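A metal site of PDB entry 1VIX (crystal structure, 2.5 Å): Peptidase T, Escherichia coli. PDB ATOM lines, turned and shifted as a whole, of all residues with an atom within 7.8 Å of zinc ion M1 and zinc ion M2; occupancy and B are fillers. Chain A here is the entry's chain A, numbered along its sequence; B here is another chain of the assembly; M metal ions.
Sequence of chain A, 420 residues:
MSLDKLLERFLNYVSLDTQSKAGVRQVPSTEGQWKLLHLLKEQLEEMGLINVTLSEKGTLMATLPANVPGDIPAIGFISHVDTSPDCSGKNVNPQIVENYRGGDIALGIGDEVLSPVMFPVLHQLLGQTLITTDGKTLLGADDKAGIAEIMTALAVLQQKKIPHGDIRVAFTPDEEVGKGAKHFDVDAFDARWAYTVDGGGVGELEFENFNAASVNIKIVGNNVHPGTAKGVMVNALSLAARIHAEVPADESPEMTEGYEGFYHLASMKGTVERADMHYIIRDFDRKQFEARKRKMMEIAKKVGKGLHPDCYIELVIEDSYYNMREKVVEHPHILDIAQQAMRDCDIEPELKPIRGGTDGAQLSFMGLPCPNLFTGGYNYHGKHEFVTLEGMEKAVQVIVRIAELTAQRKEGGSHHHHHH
The backbone NH (N) of Glu 176 sits at hydrogen-bond distance from the side-chain carboxylate (OD2) of Asp 82.
A ring nitrogen (NE2) of His 80 lies close to the side-chain carboxylate (OE1) of Glu 175, at 3.2 Å.
OD1 of Asp 143 lies within hydrogen-bond range of N of His 80 (3.1 Å).
O of Asp 82 sits at hydrogen-bond distance from ND1 of His 80 (3.1 Å).
The backbone NH (N) of Asp 142 sits at hydrogen-bond distance from the side-chain carboxylate (OE2) of Glu 385 (2.9 Å).
O of Asp 198 sits at hydrogen-bond distance from ND2 of Asn 372, at 3.1 Å.
The backbone carbonyl oxygen of Val 197 sits close to the side-chain carboxylate of Asp 143 (2.6 Å).
OG of Ser 79 sits at hydrogen-bond distance from OD1 of Asp 143, 2.8 Å away.
OE1 of Glu 175 touches zinc ion M1, at 3.999 Å.
Within 4 Å of zinc ion M1: Asp 142, Glu 175, Glu 176 and His 381.
Residues that only touch zinc ion M2: Asp 143 and Glu 175.
Within 4 Å of zinc ion M2: His 80, Asp 142, Asp 143, Glu 175, Glu 176 and Asp 198.
Zinc ion M1 is bound by OE1 of Glu 176 (2.0 Å), OD1 of Asp 142 (2.2 Å) and NE2 of His 381 (2.5 Å).
Zinc ion M1 has three donor atoms within binding distance.
NE2 of His 80 is bound to zinc ion M2 (2.1 Å).
Zinc ion M2 is bound by OD2 of Asp 142 (2.1 Å).
Zinc ion M2 is bound by OD1 of Asp 198 (2.1 Å).
Zinc ion M2 is bound by OD2 of Asp 198 (2.2 Å).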
ATOM      1  N   SER A  79     -14.845  22.128  21.281  1.00  0.00           N
ATOM      2  CA  SER A  79     -15.074  23.013  22.425  1.00  0.00           C
ATOM      3  C   SER A  79     -16.542  22.899  22.836  1.00  0.00           C
ATOM      4  O   SER A  79     -17.357  22.426  22.067  1.00  0.00           O
ATOM      5  CB  SER A  79     -14.715  24.469  22.095  1.00  0.00           C
ATOM      6  OG  SER A  79     -13.352  24.748  22.405  1.00  0.00           O
ATOM      7  N   HIS A  80     -16.866  23.293  24.059  1.00  0.00           N
ATOM      8  CA  HIS A  80     -18.260  23.214  24.497  1.00  0.00           C
ATOM      9  C   HIS A  80     -18.896  24.607  24.588  1.00  0.00           C
ATOM     10  O   HIS A  80     -18.211  25.589  24.912  1.00  0.00           O
ATOM     11  CB  HIS A  80     -18.370  22.443  25.805  1.00  0.00           C
ATOM     12  CG  HIS A  80     -17.613  23.044  26.950  1.00  0.00           C
ATOM     13  ND1 HIS A  80     -18.158  24.001  27.772  1.00  0.00           N
ATOM     14  CD2 HIS A  80     -16.365  22.819  27.417  1.00  0.00           C
ATOM     15  CE1 HIS A  80     -17.276  24.344  28.698  1.00  0.00           C
ATOM     16  NE2 HIS A  80     -16.174  23.639  28.495  1.00  0.00           N
ATOM     17  N   ASP A  82     -21.498  25.651  26.499  1.00  0.00           N
ATOM     18  CA  ASP A  82     -22.147  26.003  27.754  1.00  0.00           C
ATOM     19  C   ASP A  82     -21.171  26.564  28.773  1.00  0.00           C
ATOM     20  O   ASP A  82     -19.967  26.308  28.693  1.00  0.00           O
ATOM     21  CB  ASP A  82     -22.868  24.795  28.356  1.00  0.00           C
ATOM     22  CG  ASP A  82     -21.921  23.661  28.658  1.00  0.00           C
ATOM     23  OD1 ASP A  82     -21.172  23.258  27.734  1.00  0.00           O
ATOM     24  OD2 ASP A  82     -21.851  23.099  29.771  1.00  0.00           O
ATOM     25  N   THR A  83     -21.699  27.330  29.734  1.00  0.00           N
ATOM     26  CA  THR A  83     -20.912  27.804  30.864  1.00  0.00           C
ATOM     27  C   THR A  83     -21.443  27.218  32.166  1.00  0.00           C
ATOM     28  O   THR A  83     -22.558  26.723  32.214  1.00  0.00           O
ATOM     29  CB  THR A  83     -20.870  29.347  30.912  1.00  0.00           C
ATOM     30  OG1 THR A  83     -22.196  29.883  30.777  1.00  0.00           O
ATOM     31  CG2 THR A  83     -20.131  29.894  29.704  1.00  0.00           C
ATOM     32  N   SER A  84     -20.631  27.274  33.230  1.00  0.00           N
ATOM     33  CA  SER A  84     -20.921  26.584  34.487  1.00  0.00           C
ATOM     34  C   SER A  84     -22.182  27.064  35.221  1.00  0.00           C
ATOM     35  O   SER A  84     -22.516  28.248  35.180  1.00  0.00           O
ATOM     36  CB  SER A  84     -19.723  26.680  35.434  1.00  0.00           C
ATOM     37  OG  SER A  84     -19.956  25.916  36.602  1.00  0.00           O
ATOM     38  N   ALA A 141     -14.816  32.403  29.418  1.00  0.00           N
ATOM     39  CA  ALA A 141     -13.610  32.069  28.657  1.00  0.00           C
ATOM     40  C   ALA A 141     -13.615  30.549  28.517  1.00  0.00           C
ATOM     41  O   ALA A 141     -13.270  30.000  27.477  1.00  0.00           O
ATOM     42  CB  ALA A 141     -12.371  32.536  29.385  1.00  0.00           C
ATOM     43  N   ASP A 142     -14.040  29.902  29.600  1.00  0.00           N
ATOM     44  CA  ASP A 142     -14.374  28.483  29.600  1.00  0.00           C
ATOM     45  C   ASP A 142     -15.835  28.376  29.186  1.00  0.00           C
ATOM     46  O   ASP A 142     -16.728  28.635  29.992  1.00  0.00           O
ATOM     47  CB  ASP A 142     -14.189  27.922  31.008  1.00  0.00           C
ATOM     48  CG  ASP A 142     -14.359  26.436  31.053  1.00  0.00           C
ATOM     49  OD1 ASP A 142     -14.096  25.851  32.127  1.00  0.00           O
ATOM     50  OD2 ASP A 142     -14.754  25.747  30.087  1.00  0.00           O
ATOM     51  N   ASP A 143     -16.109  28.019  27.933  1.00  0.00           N
ATOM     52  CA  ASP A 143     -15.110  27.625  26.949  1.00  0.00           C
ATOM     53  C   ASP A 143     -15.330  28.406  25.662  1.00  0.00           C
ATOM     54  O   ASP A 143     -15.055  27.928  24.557  1.00  0.00           O
ATOM     55  CB  ASP A 143     -15.211  26.114  26.689  1.00  0.00           C
ATOM     56  CG  ASP A 143     -14.059  25.583  25.861  1.00  0.00           C
ATOM     57  OD1 ASP A 143     -14.302  24.655  25.048  1.00  0.00           O
ATOM     58  OD2 ASP A 143     -12.886  26.022  25.949  1.00  0.00           O
ATOM     59  N   LYS A 144     -15.838  29.626  25.804  1.00  0.00           N
ATOM     60  CA  LYS A 144     -16.130  30.471  24.642  1.00  0.00           C
ATOM     61  C   LYS A 144     -14.862  31.111  24.059  1.00  0.00           C
ATOM     62  O   LYS A 144     -14.855  31.589  22.918  1.00  0.00           O
ATOM     63  CB  LYS A 144     -17.176  31.519  25.003  1.00  0.00           C
ATOM     64  CG  LYS A 144     -18.546  30.940  25.265  1.00  0.00           C
ATOM     65  CD  LYS A 144     -19.377  31.852  26.165  1.00  0.00           C
ATOM     66  CE  LYS A 144     -20.829  31.439  26.148  1.00  0.00           C
ATOM     67  NZ  LYS A 144     -21.656  32.222  27.109  1.00  0.00           N
ATOM     68  N   GLU A 175     -21.246  20.019  28.570  1.00  0.00           N
ATOM     69  CA  GLU A 175     -19.980  19.625  29.155  1.00  0.00           C
ATOM     70  C   GLU A 175     -19.891  19.850  30.668  1.00  0.00           C
ATOM     71  O   GLU A 175     -19.384  18.986  31.385  1.00  0.00           O
ATOM     72  CB  GLU A 175     -18.821  20.328  28.461  1.00  0.00           C
ATOM     73  CG  GLU A 175     -17.457  19.712  28.714  1.00  0.00           C
ATOM     74  CD  GLU A 175     -16.837  20.160  30.028  1.00  0.00           C
ATOM     75  OE1 GLU A 175     -17.098  21.303  30.467  1.00  0.00           O
ATOM     76  OE2 GLU A 175     -16.093  19.353  30.629  1.00  0.00           O
ATOM     77  N   GLU A 176     -20.381  20.993  31.143  1.00  0.00           N
ATOM     78  CA  GLU A 176     -20.290  21.328  32.565  1.00  0.00           C
ATOM     79  C   GLU A 176     -21.265  20.550  33.460  1.00  0.00           C
ATOM     80  O   GLU A 176     -21.302  20.767  34.673  1.00  0.00           O
ATOM     81  CB  GLU A 176     -20.463  22.833  32.801  1.00  0.00           C
ATOM     82  CG  GLU A 176     -19.382  23.718  32.169  1.00  0.00           C
ATOM     83  CD  GLU A 176     -18.058  23.676  32.912  1.00  0.00           C
ATOM     84  OE1 GLU A 176     -17.011  23.653  32.221  1.00  0.00           O
ATOM     85  OE2 GLU A 176     -18.048  23.685  34.168  1.00  0.00           O
ATOM     86  N   THR A 196      -9.457  18.801  22.573  1.00  0.00           N
ATOM     87  CA  THR A 196     -10.372  19.795  23.116  1.00  0.00           C
ATOM     88  C   THR A 196      -9.591  21.070  23.387  1.00  0.00           C
ATOM     89  O   THR A 196      -8.479  21.027  23.928  1.00  0.00           O
ATOM     90  CB  THR A 196     -11.079  19.335  24.413  1.00  0.00           C
ATOM     91  OG1 THR A 196     -10.106  18.870  25.359  1.00  0.00           O
ATOM     92  CG2 THR A 196     -11.983  18.134  24.143  1.00  0.00           C
ATOM     93  N   VAL A 197     -10.167  22.191  23.003  1.00  0.00           N
ATOM     94  CA  VAL A 197      -9.571  23.478  23.314  1.00  0.00           C
ATOM     95  C   VAL A 197     -10.326  23.976  24.536  1.00  0.00           C
ATOM     96  O   VAL A 197     -11.262  24.760  24.440  1.00  0.00           O
ATOM     97  CB  VAL A 197      -9.633  24.428  22.089  1.00  0.00           C
ATOM     98  CG1 VAL A 197      -8.874  25.707  22.362  1.00  0.00           C
ATOM     99  CG2 VAL A 197      -9.060  23.740  20.860  1.00  0.00           C
ATOM    100  N   ASP A 198      -9.903  23.474  25.701  1.00  0.00           N
ATOM    101  CA  ASP A 198     -10.597  23.690  26.968  1.00  0.00           C
ATOM    102  C   ASP A 198      -9.633  23.653  28.158  1.00  0.00           C
ATOM    103  O   ASP A 198     -10.036  23.376  29.291  1.00  0.00           O
ATOM    104  CB  ASP A 198     -11.694  22.628  27.123  1.00  0.00           C
ATOM    105  CG  ASP A 198     -12.701  22.985  28.199  1.00  0.00           C
ATOM    106  OD1 ASP A 198     -12.934  24.183  28.437  1.00  0.00           O
ATOM    107  OD2 ASP A 198     -13.313  22.128  28.870  1.00  0.00           O
ATOM    108  N   GLY A 199      -8.357  23.945  27.885  1.00  0.00           N
ATOM    109  CA  GLY A 199      -7.335  24.015  28.917  1.00  0.00           C
ATOM    110  C   GLY A 199      -7.238  25.414  29.491  1.00  0.00           C
ATOM    111  O   GLY A 199      -8.159  26.221  29.336  1.00  0.00           O
ATOM    112  N   GLY A 357     -12.629  14.735  35.246  1.00  0.00           N
ATOM    113  CA  GLY A 357     -12.922  14.225  33.918  1.00  0.00           C
ATOM    114  C   GLY A 357     -13.073  15.307  32.877  1.00  0.00           C
ATOM    115  O   GLY A 357     -13.297  16.485  33.203  1.00  0.00           O
ATOM    116  N   THR A 358     -12.927  14.921  31.612  1.00  0.00           N
ATOM    117  CA  THR A 358     -13.212  15.802  30.486  1.00  0.00           C
ATOM    118  C   THR A 358     -14.069  15.053  29.471  1.00  0.00           C
ATOM    119  O   THR A 358     -14.261  13.839  29.602  1.00  0.00           O
ATOM    120  CB  THR A 358     -11.914  16.291  29.813  1.00  0.00           C
ATOM    121  OG1 THR A 358     -10.940  15.240  29.841  1.00  0.00           O
ATOM    122  CG2 THR A 358     -11.273  17.417  30.635  1.00  0.00           C
ATOM    123  N   ASP A 359     -14.580  15.789  28.494  1.00  0.00           N
ATOM    124  CA  ASP A 359     -15.263  15.205  27.334  1.00  0.00           C
ATOM    125  C   ASP A 359     -14.294  14.314  26.580  1.00  0.00           C
ATOM    126  O   ASP A 359     -14.661  13.220  26.142  1.00  0.00           O
ATOM    127  CB  ASP A 359     -15.753  16.301  26.407  1.00  0.00           C
ATOM    128  CG  ASP A 359     -17.067  16.863  26.817  1.00  0.00           C
ATOM    129  OD1 ASP A 359     -17.539  17.808  26.147  1.00  0.00           O
ATOM    130  OD2 ASP A 359     -17.712  16.442  27.808  1.00  0.00           O
ATOM    131  N   ASN A 372      -6.254  17.607  25.944  1.00  0.00           N
ATOM    132  CA  ASN A 372      -6.779  18.957  26.157  1.00  0.00           C
ATOM    133  C   ASN A 372      -5.737  20.049  25.899  1.00  0.00           C
ATOM    134  O   ASN A 372      -4.609  19.921  26.337  1.00  0.00           O
ATOM    135  CB  ASN A 372      -7.346  19.103  27.574  1.00  0.00           C
ATOM    136  CG  ASN A 372      -8.300  20.267  27.715  1.00  0.00           C
ATOM    137  OD1 ASN A 372      -8.967  20.664  26.747  1.00  0.00           O
ATOM    138  ND2 ASN A 372      -8.382  20.831  28.912  1.00  0.00           N
ATOM    139  N   THR A 375      -6.309  27.545  26.559  1.00  0.00           N
ATOM    140  CA  THR A 375      -7.224  28.556  26.084  1.00  0.00           C
ATOM    141  C   THR A 375      -6.681  29.967  26.380  1.00  0.00           C
ATOM    142  O   THR A 375      -6.998  30.935  25.681  1.00  0.00           O
ATOM    143  CB  THR A 375      -8.579  28.334  26.755  1.00  0.00           C
ATOM    144  OG1 THR A 375      -9.411  27.555  25.897  1.00  0.00           O
ATOM    145  CG2 THR A 375      -9.336  29.602  26.895  1.00  0.00           C
ATOM    146  N   TYR A 380     -11.539  29.540  36.343  1.00  0.00           N
ATOM    147  CA  TYR A 380     -12.808  29.138  35.744  1.00  0.00           C
ATOM    148  C   TYR A 380     -13.884  28.856  36.788  1.00  0.00           C
ATOM    149  O   TYR A 380     -13.573  28.471  37.916  1.00  0.00           O
ATOM    150  CB  TYR A 380     -12.587  27.924  34.843  1.00  0.00           C
ATOM    151  CG  TYR A 380     -11.712  28.210  33.633  1.00  0.00           C
ATOM    152  CD1 TYR A 380     -10.827  27.257  33.144  1.00  0.00           C
ATOM    153  CD2 TYR A 380     -11.781  29.455  32.965  1.00  0.00           C
ATOM    154  CE1 TYR A 380     -10.022  27.517  32.025  1.00  0.00           C
ATOM    155  CE2 TYR A 380     -10.998  29.719  31.849  1.00  0.00           C
ATOM    156  CZ  TYR A 380     -10.127  28.746  31.386  1.00  0.00           C
ATOM    157  OH  TYR A 380      -9.349  28.999  30.279  1.00  0.00           O
ATOM    158  N   HIS A 381     -15.141  29.075  36.402  1.00  0.00           N
ATOM    159  CA  HIS A 381     -16.314  28.771  37.241  1.00  0.00           C
ATOM    160  C   HIS A 381     -16.484  29.710  38.439  1.00  0.00           C
ATOM    161  O   HIS A 381     -16.667  29.266  39.582  1.00  0.00           O
ATOM    162  CB  HIS A 381     -16.333  27.290  37.669  1.00  0.00           C
ATOM    163  CG  HIS A 381     -15.997  26.329  36.572  1.00  0.00           C
ATOM    164  ND1 HIS A 381     -15.313  25.152  36.791  1.00  0.00           N
ATOM    165  CD2 HIS A 381     -16.238  26.372  35.236  1.00  0.00           C
ATOM    166  CE1 HIS A 381     -15.158  24.517  35.650  1.00  0.00           C
ATOM    167  NE2 HIS A 381     -15.710  25.239  34.690  1.00  0.00           N
ATOM    168  N   GLU A 385     -12.929  35.010  36.942  1.00  0.00           N
ATOM    169  CA  GLU A 385     -12.501  34.449  35.655  1.00  0.00           C
ATOM    170  C   GLU A 385     -11.973  35.542  34.727  1.00  0.00           C
ATOM    171  O   GLU A 385     -12.637  36.562  34.500  1.00  0.00           O
ATOM    172  CB  GLU A 385     -13.628  33.667  34.990  1.00  0.00           C
ATOM    173  CG  GLU A 385     -13.108  32.674  33.967  1.00  0.00           C
ATOM    174  CD  GLU A 385     -14.173  32.186  33.003  1.00  0.00           C
ATOM    175  OE1 GLU A 385     -15.383  32.417  33.240  1.00  0.00           O
ATOM    176  OE2 GLU A 385     -13.794  31.565  32.005  1.00  0.00           O
ATOM    177  N   HIS B 225     -15.066  22.244  43.374  1.00  0.00           N
ATOM    178  CA  HIS B 225     -14.751  21.039  42.613  1.00  0.00           C
ATOM    179  C   HIS B 225     -13.622  20.310  43.342  1.00  0.00           C
ATOM    180  O   HIS B 225     -12.553  20.892  43.546  1.00  0.00           O
ATOM    181  CB  HIS B 225     -14.325  21.393  41.182  1.00  0.00           C
ATOM    182  CG  HIS B 225     -15.455  21.751  40.273  1.00  0.00           C
ATOM    183  ND1 HIS B 225     -15.286  22.514  39.134  1.00  0.00           N
ATOM    184  CD2 HIS B 225     -16.775  21.420  40.305  1.00  0.00           C
ATOM    185  CE1 HIS B 225     -16.446  22.656  38.515  1.00  0.00           C
ATOM    186  NE2 HIS B 225     -17.368  21.999  39.210  1.00  0.00           N
HETATM  187 ZN    ZN M   1     -15.029  23.968  32.613  1.00  0.00          ZN
HETATM  188 ZN    ZN M   2     -14.518  23.732  29.710  1.00  0.00          ZN
